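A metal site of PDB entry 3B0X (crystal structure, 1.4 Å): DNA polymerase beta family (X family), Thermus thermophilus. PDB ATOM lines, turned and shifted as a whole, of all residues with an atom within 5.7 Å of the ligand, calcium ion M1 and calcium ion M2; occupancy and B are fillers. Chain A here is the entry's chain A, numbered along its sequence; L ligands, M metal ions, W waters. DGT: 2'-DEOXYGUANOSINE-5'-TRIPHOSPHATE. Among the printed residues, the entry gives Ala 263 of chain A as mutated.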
ATOM      1  N   MET A   1     -28.011 -21.945  -3.925  1.00  0.00           N
ATOM      2  CA  MET A   1     -26.900 -22.478  -3.081  1.00  0.00           C
ATOM      3  C   MET A   1     -26.942 -21.935  -1.668  1.00  0.00           C
ATOM      4  O   MET A   1     -27.331 -20.785  -1.447  1.00  0.00           O
ATOM      5  CB  MET A   1     -25.547 -22.152  -3.710  1.00  0.00           C
ATOM      6  CG  MET A   1     -25.097 -23.180  -4.713  1.00  0.00           C
ATOM      7  SD  MET A   1     -23.372 -22.936  -5.147  1.00  0.00           S
ATOM      8  CE  MET A   1     -23.554 -21.923  -6.612  1.00  0.00           C
ATOM      9  N   ARG A 157     -29.073   2.552   1.698  1.00  0.00           N
ATOM     10  CA  ARG A 157     -29.064   2.693   0.231  1.00  0.00           C
ATOM     11  C   ARG A 157     -28.730   4.127  -0.134  1.00  0.00           C
ATOM     12  O   ARG A 157     -29.000   5.032   0.646  1.00  0.00           O
ATOM     13  CB  ARG A 157     -30.404   2.250  -0.350  1.00  0.00           C
ATOM     14  CG  ARG A 157     -30.811   0.851   0.132  1.00  0.00           C
ATOM     15  CD  ARG A 157     -32.099   0.367  -0.499  1.00  0.00           C
ATOM     16  NE  ARG A 157     -31.951   0.130  -1.933  1.00  0.00           N
ATOM     17  CZ  ARG A 157     -31.428  -0.957  -2.472  1.00  0.00           C
ATOM     18  NH1 ARG A 157     -31.007  -1.965  -1.719  1.00  0.00           N
ATOM     19  NH2 ARG A 157     -31.362  -1.071  -3.787  1.00  0.00           N
ATOM     20  N   CYS A 186     -22.539  -4.386 -12.564  1.00  0.00           N
ATOM     21  CA  CYS A 186     -23.769  -5.158 -12.619  1.00  0.00           C
ATOM     22  C   CYS A 186     -24.701  -4.792 -11.459  1.00  0.00           C
ATOM     23  O   CYS A 186     -24.835  -3.612 -11.120  1.00  0.00           O
ATOM     24  CB  CYS A 186     -23.440  -6.658 -12.719  1.00  0.00           C
ATOM     25  SG  CYS A 186     -22.519  -7.093 -14.228  1.00  0.00           S
ATOM     26  N   GLY A 187     -25.348  -5.783 -10.863  1.00  0.00           N
ATOM     27  CA  GLY A 187     -26.292  -5.575  -9.775  1.00  0.00           C
ATOM     28  C   GLY A 187     -27.394  -4.599 -10.135  1.00  0.00           C
ATOM     29  O   GLY A 187     -27.710  -4.345 -11.313  1.00  0.00           O
ATOM     30  N   SER A 188     -27.990  -4.013  -9.102  1.00  0.00           N
ATOM     31  CA  SER A 188     -29.145  -3.116  -9.287  1.00  0.00           C
ATOM     32  C   SER A 188     -28.758  -1.825 -10.028  1.00  0.00           C
ATOM     33  O   SER A 188     -29.610  -1.225 -10.694  1.00  0.00           O
ATOM     34  CB  SER A 188     -29.783  -2.800  -7.954  1.00  0.00           C
ATOM     35  OG  SER A 188     -28.838  -2.154  -7.121  1.00  0.00           O
ATOM     36  N   ALA A 189     -27.475  -1.443  -9.984  1.00  0.00           N
ATOM     37  CA  ALA A 189     -27.031  -0.273 -10.727  1.00  0.00           C
ATOM     38  C   ALA A 189     -27.222  -0.477 -12.228  1.00  0.00           C
ATOM     39  O   ALA A 189     -27.666   0.437 -12.924  1.00  0.00           O
ATOM     40  CB  ALA A 189     -25.583   0.057 -10.424  1.00  0.00           C
ATOM     41  N   ARG A 191     -29.422  -2.188 -13.598  1.00  0.00           N
ATOM     42  CA  ARG A 191     -30.862  -2.161 -13.836  1.00  0.00           C
ATOM     43  C   ARG A 191     -31.454  -0.749 -13.672  1.00  0.00           C
ATOM     44  O   ARG A 191     -32.664  -0.579 -13.820  1.00  0.00           O
ATOM     45  CB  ARG A 191     -31.599  -3.155 -12.947  1.00  0.00           C
ATOM     46  CG  ARG A 191     -31.010  -4.578 -13.011  1.00  0.00           C
ATOM     47  CD  ARG A 191     -31.988  -5.634 -12.520  1.00  0.00           C
ATOM     48  NE  ARG A 191     -32.561  -5.328 -11.211  1.00  0.00           N
ATOM     49  CZ  ARG A 191     -31.991  -5.574 -10.030  1.00  0.00           C
ATOM     50  NH1 ARG A 191     -30.805  -6.171  -9.922  1.00  0.00           N
ATOM     51  NH2 ARG A 191     -32.617  -5.176  -8.900  1.00  0.00           N
ATOM     52  N   LYS A 193     -31.968   0.956 -11.017  1.00  0.00           N
ATOM     53  CA  LYS A 193     -32.750   1.144  -9.793  1.00  0.00           C
ATOM     54  C   LYS A 193     -32.354   2.455  -9.145  1.00  0.00           C
ATOM     55  O   LYS A 193     -31.170   2.804  -9.148  1.00  0.00           O
ATOM     56  CB  LYS A 193     -32.484  -0.013  -8.865  1.00  0.00           C
ATOM     57  CG  LYS A 193     -33.526  -0.147  -7.764  1.00  0.00           C
ATOM     58  CD  LYS A 193     -33.284  -1.415  -6.958  1.00  0.00           C
ATOM     59  CE  LYS A 193     -34.246  -1.531  -5.792  1.00  0.00           C
ATOM     60  NZ  LYS A 193     -35.585  -1.948  -6.322  1.00  0.00           N
ATOM     61  N   THR A 195     -32.181   3.664  -6.102  1.00  0.00           N
ATOM     62  CA  THR A 195     -31.282   3.617  -4.956  1.00  0.00           C
ATOM     63  C   THR A 195     -30.613   2.263  -5.018  1.00  0.00           C
ATOM     64  O   THR A 195     -31.199   1.286  -5.510  1.00  0.00           O
ATOM     65  CB  THR A 195     -31.975   3.800  -3.594  1.00  0.00           C
ATOM     66  OG1 THR A 195     -32.778   2.661  -3.275  1.00  0.00           O
ATOM     67  CG2 THR A 195     -32.810   5.091  -3.564  1.00  0.00           C
ATOM     68  N   VAL A 196     -29.386   2.196  -4.518  1.00  0.00           N
ATOM     69  CA  VAL A 196     -28.589   0.978  -4.595  1.00  0.00           C
ATOM     70  C   VAL A 196     -27.987   0.647  -3.254  1.00  0.00           C
ATOM     71  O   VAL A 196     -27.661   1.549  -2.466  1.00  0.00           O
ATOM     72  CB  VAL A 196     -27.495   1.067  -5.681  1.00  0.00           C
ATOM     73  CG1 VAL A 196     -28.125   1.236  -7.055  1.00  0.00           C
ATOM     74  CG2 VAL A 196     -26.511   2.205  -5.371  1.00  0.00           C
ATOM     75  N   GLY A 197     -27.801  -0.645  -3.020  1.00  0.00           N
ATOM     76  CA  GLY A 197     -26.996  -1.127  -1.891  1.00  0.00           C
ATOM     77  C   GLY A 197     -25.556  -1.157  -2.329  1.00  0.00           C
ATOM     78  O   GLY A 197     -25.027  -0.196  -2.883  1.00  0.00           O
ATOM     79  N   ASP A 198     -24.882  -2.275  -2.080  1.00  0.00           N
ATOM     80  CA  ASP A 198     -23.498  -2.394  -2.531  1.00  0.00           C
ATOM     81  C   ASP A 198     -23.392  -2.406  -4.066  1.00  0.00           C
ATOM     82  O   ASP A 198     -24.396  -2.581  -4.771  1.00  0.00           O
ATOM     83  CB  ASP A 198     -22.784  -3.591  -1.897  1.00  0.00           C
ATOM     84  CG  ASP A 198     -23.336  -4.934  -2.359  1.00  0.00           C
ATOM     85  OD1 ASP A 198     -24.073  -5.024  -3.365  1.00  0.00           O
ATOM     86  OD2 ASP A 198     -23.028  -5.945  -1.705  1.00  0.00           O
ATOM     87  N   LEU A 199     -22.183  -2.141  -4.564  1.00  0.00           N
ATOM     88  CA  LEU A 199     -21.934  -2.183  -6.008  1.00  0.00           C
ATOM     89  C   LEU A 199     -21.276  -3.487  -6.366  1.00  0.00           C
ATOM     90  O   LEU A 199     -20.450  -3.978  -5.607  1.00  0.00           O
ATOM     91  CB  LEU A 199     -21.041  -1.030  -6.418  1.00  0.00           C
ATOM     92  CG  LEU A 199     -21.784   0.298  -6.198  1.00  0.00           C
ATOM     93  CD1 LEU A 199     -20.754   1.384  -6.111  1.00  0.00           C
ATOM     94  CD2 LEU A 199     -22.808   0.619  -7.257  1.00  0.00           C
ATOM     95  N   ASP A 200     -21.663  -4.069  -7.505  1.00  0.00           N
ATOM     96  CA  ASP A 200     -21.223  -5.405  -7.881  1.00  0.00           C
ATOM     97  C   ASP A 200     -20.578  -5.344  -9.244  1.00  0.00           C
ATOM     98  O   ASP A 200     -21.205  -4.840 -10.188  1.00  0.00           O
ATOM     99  CB  ASP A 200     -22.444  -6.330  -7.954  1.00  0.00           C
ATOM    100  CG  ASP A 200     -23.250  -6.267  -6.703  1.00  0.00           C
ATOM    101  OD1 ASP A 200     -22.921  -7.013  -5.771  1.00  0.00           O
ATOM    102  OD2 ASP A 200     -24.196  -5.464  -6.638  1.00  0.00           O
ATOM    103  N   ASP A 243     -18.538  -5.510  -4.243  1.00  0.00           N
ATOM    104  CA  ASP A 243     -18.331  -6.909  -4.483  1.00  0.00           C
ATOM    105  C   ASP A 243     -17.762  -7.097  -5.889  1.00  0.00           C
ATOM    106  O   ASP A 243     -18.219  -6.468  -6.856  1.00  0.00           O
ATOM    107  CB  ASP A 243     -19.656  -7.658  -4.454  1.00  0.00           C
ATOM    108  CG  ASP A 243     -20.219  -7.828  -3.073  1.00  0.00           C
ATOM    109  OD1 ASP A 243     -19.517  -7.692  -2.057  1.00  0.00           O
ATOM    110  OD2 ASP A 243     -21.437  -8.141  -2.988  1.00  0.00           O
ATOM    111  N   TYR A 258     -26.103 -13.460 -14.283  1.00  0.00           N
ATOM    112  CA  TYR A 258     -26.117 -13.802 -12.873  1.00  0.00           C
ATOM    113  C   TYR A 258     -26.009 -12.552 -11.991  1.00  0.00           C
ATOM    114  O   TYR A 258     -26.797 -12.349 -11.055  1.00  0.00           O
ATOM    115  CB  TYR A 258     -24.995 -14.794 -12.575  1.00  0.00           C
ATOM    116  CG  TYR A 258     -24.894 -15.136 -11.123  1.00  0.00           C
ATOM    117  CD1 TYR A 258     -25.562 -16.241 -10.599  1.00  0.00           C
ATOM    118  CD2 TYR A 258     -24.150 -14.339 -10.256  1.00  0.00           C
ATOM    119  CE1 TYR A 258     -25.488 -16.536  -9.237  1.00  0.00           C
ATOM    120  CE2 TYR A 258     -24.075 -14.611  -8.900  1.00  0.00           C
ATOM    121  CZ  TYR A 258     -24.738 -15.716  -8.404  1.00  0.00           C
ATOM    122  OH  TYR A 258     -24.670 -16.015  -7.057  1.00  0.00           O
ATOM    123  N   LEU A 259     -24.978 -11.755 -12.237  1.00  0.00           N
ATOM    124  CA  LEU A 259     -24.692 -10.655 -11.328  1.00  0.00           C
ATOM    125  C   LEU A 259     -25.595  -9.437 -11.514  1.00  0.00           C
ATOM    126  O   LEU A 259     -25.632  -8.529 -10.663  1.00  0.00           O
ATOM    127  CB  LEU A 259     -23.215 -10.268 -11.421  1.00  0.00           C
ATOM    128  CG  LEU A 259     -22.657  -9.502 -10.223  1.00  0.00           C
ATOM    129  CD1 LEU A 259     -22.901 -10.208  -8.939  1.00  0.00           C
ATOM    130  CD2 LEU A 259     -21.190  -9.188 -10.435  1.00  0.00           C
ATOM    131  N   THR A 260     -26.336  -9.408 -12.618  1.00  0.00           N
ATOM    132  CA  THR A 260     -27.282  -8.308 -12.874  1.00  0.00           C
ATOM    133  C   THR A 260     -28.636  -8.564 -12.236  1.00  0.00           C
ATOM    134  O   THR A 260     -29.320  -7.628 -11.825  1.00  0.00           O
ATOM    135  CB  THR A 260     -27.405  -8.059 -14.390  1.00  0.00           C
ATOM    136  OG1 THR A 260     -26.113  -7.661 -14.884  1.00  0.00           O
ATOM    137  CG2 THR A 260     -28.406  -6.973 -14.729  1.00  0.00           C
ATOM    138  N   GLY A 261     -29.018  -9.831 -12.148  1.00  0.00           N
ATOM    139  CA  GLY A 261     -30.307 -10.176 -11.566  1.00  0.00           C
ATOM    140  C   GLY A 261     -31.439  -9.476 -12.308  1.00  0.00           C
ATOM    141  O   GLY A 261     -31.379  -9.290 -13.513  1.00  0.00           O
ATOM    142  N   SER A 262     -32.518  -9.077 -11.619  1.00  0.00           N
ATOM    143  CA  SER A 262     -32.749  -9.341 -10.211  1.00  0.00           C
ATOM    144  C   SER A 262     -32.781 -10.840  -9.908  1.00  0.00           C
ATOM    145  O   SER A 262     -32.895 -11.689 -10.821  1.00  0.00           O
ATOM    146  CB  SER A 262     -34.079  -8.739  -9.827  1.00  0.00           C
ATOM    147  OG  SER A 262     -35.149  -9.500 -10.377  1.00  0.00           O
ATOM    148  N   ALA A 263     -32.718 -11.193  -8.636  1.00  0.00           N
ATOM    149  CA  ALA A 263     -32.825 -12.597  -8.244  1.00  0.00           C
ATOM    150  C   ALA A 263     -34.116 -13.210  -8.772  1.00  0.00           C
ATOM    151  O   ALA A 263     -34.105 -14.368  -9.226  1.00  0.00           O
ATOM    152  CB  ALA A 263     -32.724 -12.755  -6.721  1.00  0.00           C
ATOM    153  N   SER A 266     -33.708 -14.069 -12.416  1.00  0.00           N
ATOM    154  CA  SER A 266     -32.883 -15.255 -12.595  1.00  0.00           C
ATOM    155  C   SER A 266     -33.619 -16.549 -12.240  1.00  0.00           C
ATOM    156  O   SER A 266     -33.427 -17.578 -12.895  1.00  0.00           O
ATOM    157  CB  SER A 266     -31.597 -15.170 -11.791  1.00  0.00           C
ATOM    158  OG  SER A 266     -30.867 -14.063 -12.232  1.00  0.00           O
ATOM    159  N   ARG A 270     -33.753 -19.686 -14.824  1.00  0.00           N
ATOM    160  CA  ARG A 270     -33.270 -21.029 -14.488  1.00  0.00           C
ATOM    161  C   ARG A 270     -34.342 -22.103 -14.733  1.00  0.00           C
ATOM    162  O   ARG A 270     -34.024 -23.234 -15.153  1.00  0.00           O
ATOM    163  CB  ARG A 270     -32.758 -21.117 -13.054  1.00  0.00           C
ATOM    164  CG  ARG A 270     -31.427 -20.407 -12.846  1.00  0.00           C
ATOM    165  CD  ARG A 270     -30.759 -20.859 -11.547  1.00  0.00           C
ATOM    166  NE  ARG A 270     -31.625 -20.597 -10.415  1.00  0.00           N
ATOM    167  CZ  ARG A 270     -31.720 -19.430  -9.781  1.00  0.00           C
ATOM    168  NH1 ARG A 270     -30.980 -18.400 -10.144  1.00  0.00           N
ATOM    169  NH2 ARG A 270     -32.579 -19.319  -8.775  1.00  0.00           N
HETATM  170  PG  DGT L   1     -28.982  -4.027  -4.040  1.00  0.00           P
HETATM  171  O1G DGT L   1     -27.524  -4.334  -3.787  1.00  0.00           O
HETATM  172  O2G DGT L   1     -29.916  -4.295  -2.881  1.00  0.00           O
HETATM  173  O3G DGT L   1     -29.222  -2.628  -4.603  1.00  0.00           O
HETATM  174  O3B DGT L   1     -29.514  -4.991  -5.234  1.00  0.00           O
HETATM  175  PB  DGT L   1     -28.672  -6.010  -6.130  1.00  0.00           P
HETATM  176  O1B DGT L   1     -29.600  -6.564  -7.158  1.00  0.00           O
HETATM  177  O2B DGT L   1     -27.383  -5.408  -6.588  1.00  0.00           O
HETATM  178  O3A DGT L   1     -28.377  -7.202  -5.089  1.00  0.00           O
HETATM  179  PA  DGT L   1     -27.065  -7.912  -4.495  1.00  0.00           P
HETATM  180  O1A DGT L   1     -25.914  -6.967  -4.456  1.00  0.00           O
HETATM  181  O2A DGT L   1     -27.499  -8.573  -3.209  1.00  0.00           O
HETATM  182  O5' DGT L   1     -26.783  -9.104  -5.499  1.00  0.00           O
HETATM  183  C5' DGT L   1     -26.285  -8.798  -6.822  1.00  0.00           C
HETATM  184  C4' DGT L   1     -26.880  -9.751  -7.839  1.00  0.00           C
HETATM  185  O4' DGT L   1     -26.461 -11.070  -7.521  1.00  0.00           O
HETATM  186  C3' DGT L   1     -28.384  -9.837  -7.877  1.00  0.00           C
HETATM  187  O3' DGT L   1     -28.987  -8.814  -8.656  1.00  0.00           O
HETATM  188  C2' DGT L   1     -28.632 -11.193  -8.479  1.00  0.00           C
HETATM  189  C1' DGT L   1     -27.465 -12.004  -7.929  1.00  0.00           C
HETATM  190  N9  DGT L   1     -27.871 -12.775  -6.749  1.00  0.00           N
HETATM  191  C8  DGT L   1     -27.962 -12.308  -5.477  1.00  0.00           C
HETATM  192  N7  DGT L   1     -28.368 -13.307  -4.657  1.00  0.00           N
HETATM  193  C5  DGT L   1     -28.516 -14.406  -5.419  1.00  0.00           C
HETATM  194  C6  DGT L   1     -28.922 -15.802  -5.181  1.00  0.00           C
HETATM  195  O6  DGT L   1     -29.208 -16.198  -4.031  1.00  0.00           O
HETATM  196  N1  DGT L   1     -28.947 -16.609  -6.241  1.00  0.00           N
HETATM  197  C2  DGT L   1     -28.636 -16.199  -7.494  1.00  0.00           C
HETATM  198  N2  DGT L   1     -28.704 -17.085  -8.493  1.00  0.00           N
HETATM  199  N3  DGT L   1     -28.274 -14.937  -7.817  1.00  0.00           N
HETATM  200  C4  DGT L   1     -28.182 -14.039  -6.798  1.00  0.00           C
HETATM  201 CA    CA M   1     -23.648  -7.490  -3.560  1.00  0.00          CA
HETATM  202 CA    CA M   2     -25.664  -4.643  -5.114  1.00  0.00          CA
HETATM  203  O   HOH W   1     -28.319 -19.986  -7.948  1.00  0.00           O
HETATM  204  O   HOH W   2     -32.212  -6.617  -6.504  1.00  0.00           O
HETATM  205  O   HOH W   3     -26.543  -4.553  -1.222  1.00  0.00           O
HETATM  206  O   HOH W   4     -29.952 -19.271  -5.903  1.00  0.00           O
HETATM  207  O   HOH W   5     -24.874  -8.308  -1.761  1.00  0.00           O
HETATM  208  O   HOH W   6     -28.965 -13.811 -10.391  1.00  0.00           O
HETATM  209  O   HOH W   7     -32.529  -4.807  -3.911  1.00  0.00           O
HETATM  210  O   HOH W   8     -26.889 -11.164  -2.446  1.00  0.00           O
HETATM  211  O   HOH W   9     -23.858  -9.747  -4.236  1.00  0.00           O
HETATM  212  O   HOH W  10     -28.417 -18.152 -11.418  1.00  0.00           O
HETATM  213  O   HOH W  11     -32.078 -16.193  -8.253  1.00  0.00           O
HETATM  214  O   HOH W  12     -26.181  -2.730  -6.710  1.00  0.00           O
HETATM  215  O   HOH W  13     -30.033  -8.797  -2.482  1.00  0.00           O
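An oxygen (O2B) of the ligand lies close to the backbone NH of Ser 188, at 2.9 Å.
An oxygen (O3G) of the ligand sits at hydrogen-bond distance from the side-chain hydroxyl (OG) of Ser 188.
An oxygen (O3G) of the ligand lies within salt-bridge range of the guanidinium group (NH2) of Arg 157, 2.8 Å away.
The backbone NH (N) of Gly 197 is in hydrogen-bond range of an oxygen (O3G) of the ligand, 2.9 Å away.
NH1 of Arg 191 is in salt-bridge range of O1B of the ligand (3.0 Å).
The backbone carbonyl oxygen (O) of Thr 260 is in hydrogen-bond range of an oxygen (O3') of the ligand (3.4 Å).
The backbone carbonyl oxygen (O) of Asp 200 sits at hydrogen-bond distance from the backbone NH (N) of Cys 186 (2.8 Å).
The backbone NH of Asp 243 lies within hydrogen-bond range of the backbone carbonyl oxygen of Leu 199 (2.8 Å).
O of Ser 188 lies within hydrogen-bond range of N of Lys 193 (3.2 Å).
NH2 of Arg 157 is in hydrogen-bond range of O of Thr 195.
The guanidinium group (NH1) of Arg 191 sits at hydrogen-bond distance from the backbone carbonyl oxygen (O) of Thr 260.
O of Leu 259 sits at hydrogen-bond distance from N of Gly 187 (2.8 Å).
The side-chain hydroxyl (OG1) of Thr 260 lies close to the side-chain sulfur (SG) of Cys 186 (3.7 Å).
NH1 of Arg 270 lies close to N2 of the ligand (3.1 Å).
Residues that only touch the ligand: Tyr 258 (3.2 Å), Leu 259 (3.3 Å), Gly 187 (3.4 Å), Gly 261 (3.5 Å) and Val 196 (3.7 Å).
Hydrophobic or aromatic side chains within 4 Å of the ligand: Tyr 258 and Leu 259.
Within 4 Å of the ligand: Arg 157, Gly 187, Ser 188, Arg 191, Val 196, Gly 197, Asp 198, Asp 200, Tyr 258, Leu 259, Thr 260, Gly 261 and Arg 270.
Along chain A the residues within 4 Å of the ligand span positions 157 to 270.
The nearest printed residue that does not touch the ligand is Ala 263 (4.1 Å).
Within 4 Å of calcium ion M1: Asp 198, Asp 200 and Asp 243.
The nearest printed residue that does not touch calcium ion M1 is Leu 199 (5.2 Å).
The nearest printed residue that does not touch calcium ion M2 is Leu 199 (4.3 Å).
Calcium ion M1 is bound by water W5, 2.3 Å away.
Water W9 binds calcium ion M1, at 2.4 Å.
Calcium ion M1 is bound by OD2 of Asp 243, at 2.4 Å.
OD1 of Asp 200 binds calcium ion M1 (2.4 Å).
Calcium ion M1 is bound by O1A of the ligand (2.5 Å).
Calcium ion M1 is bound by OD2 of Asp 198 (2.5 Å).
The side-chain carboxylate (OD1) of Asp 198 is bound to calcium ion M1.
Calcium ion M2 is bound by the side-chain carboxylate (OD2) of Asp 200 (2.3 Å), an oxygen (O1G) of the ligand (2.3 Å), an oxygen (O2B) of the ligand (2.4 Å), the side-chain carboxylate (OD1) of Asp 198 (2.4 Å), an oxygen (O1A) of the ligand (2.4 Å), the backbone carbonyl oxygen (O) of Asp 198 (2.4 Å) and water W12 (2.5 Å).
Water W2 bridges an oxygen (O1B) of the ligand (2.7 Å) and the guanidinium group (NH2) of Arg 191 (2.8 Å).
Water W6 lies within hydrogen-bond range of OG of Ser 266 (2.7 Å), O of Tyr 258 (2.7 Å) and N3 of the ligand (2.9 Å).
Water W10 lies within hydrogen-bond range of NH1 of Arg 270 (2.9 Å) and N2 of the ligand (3.1 Å).
Water W11 lies within hydrogen-bond range of the backbone carbonyl oxygen (O) of Ala 263, the guanidinium group (NH1) of Arg 270 and a nitrogen (N2) of the ligand.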
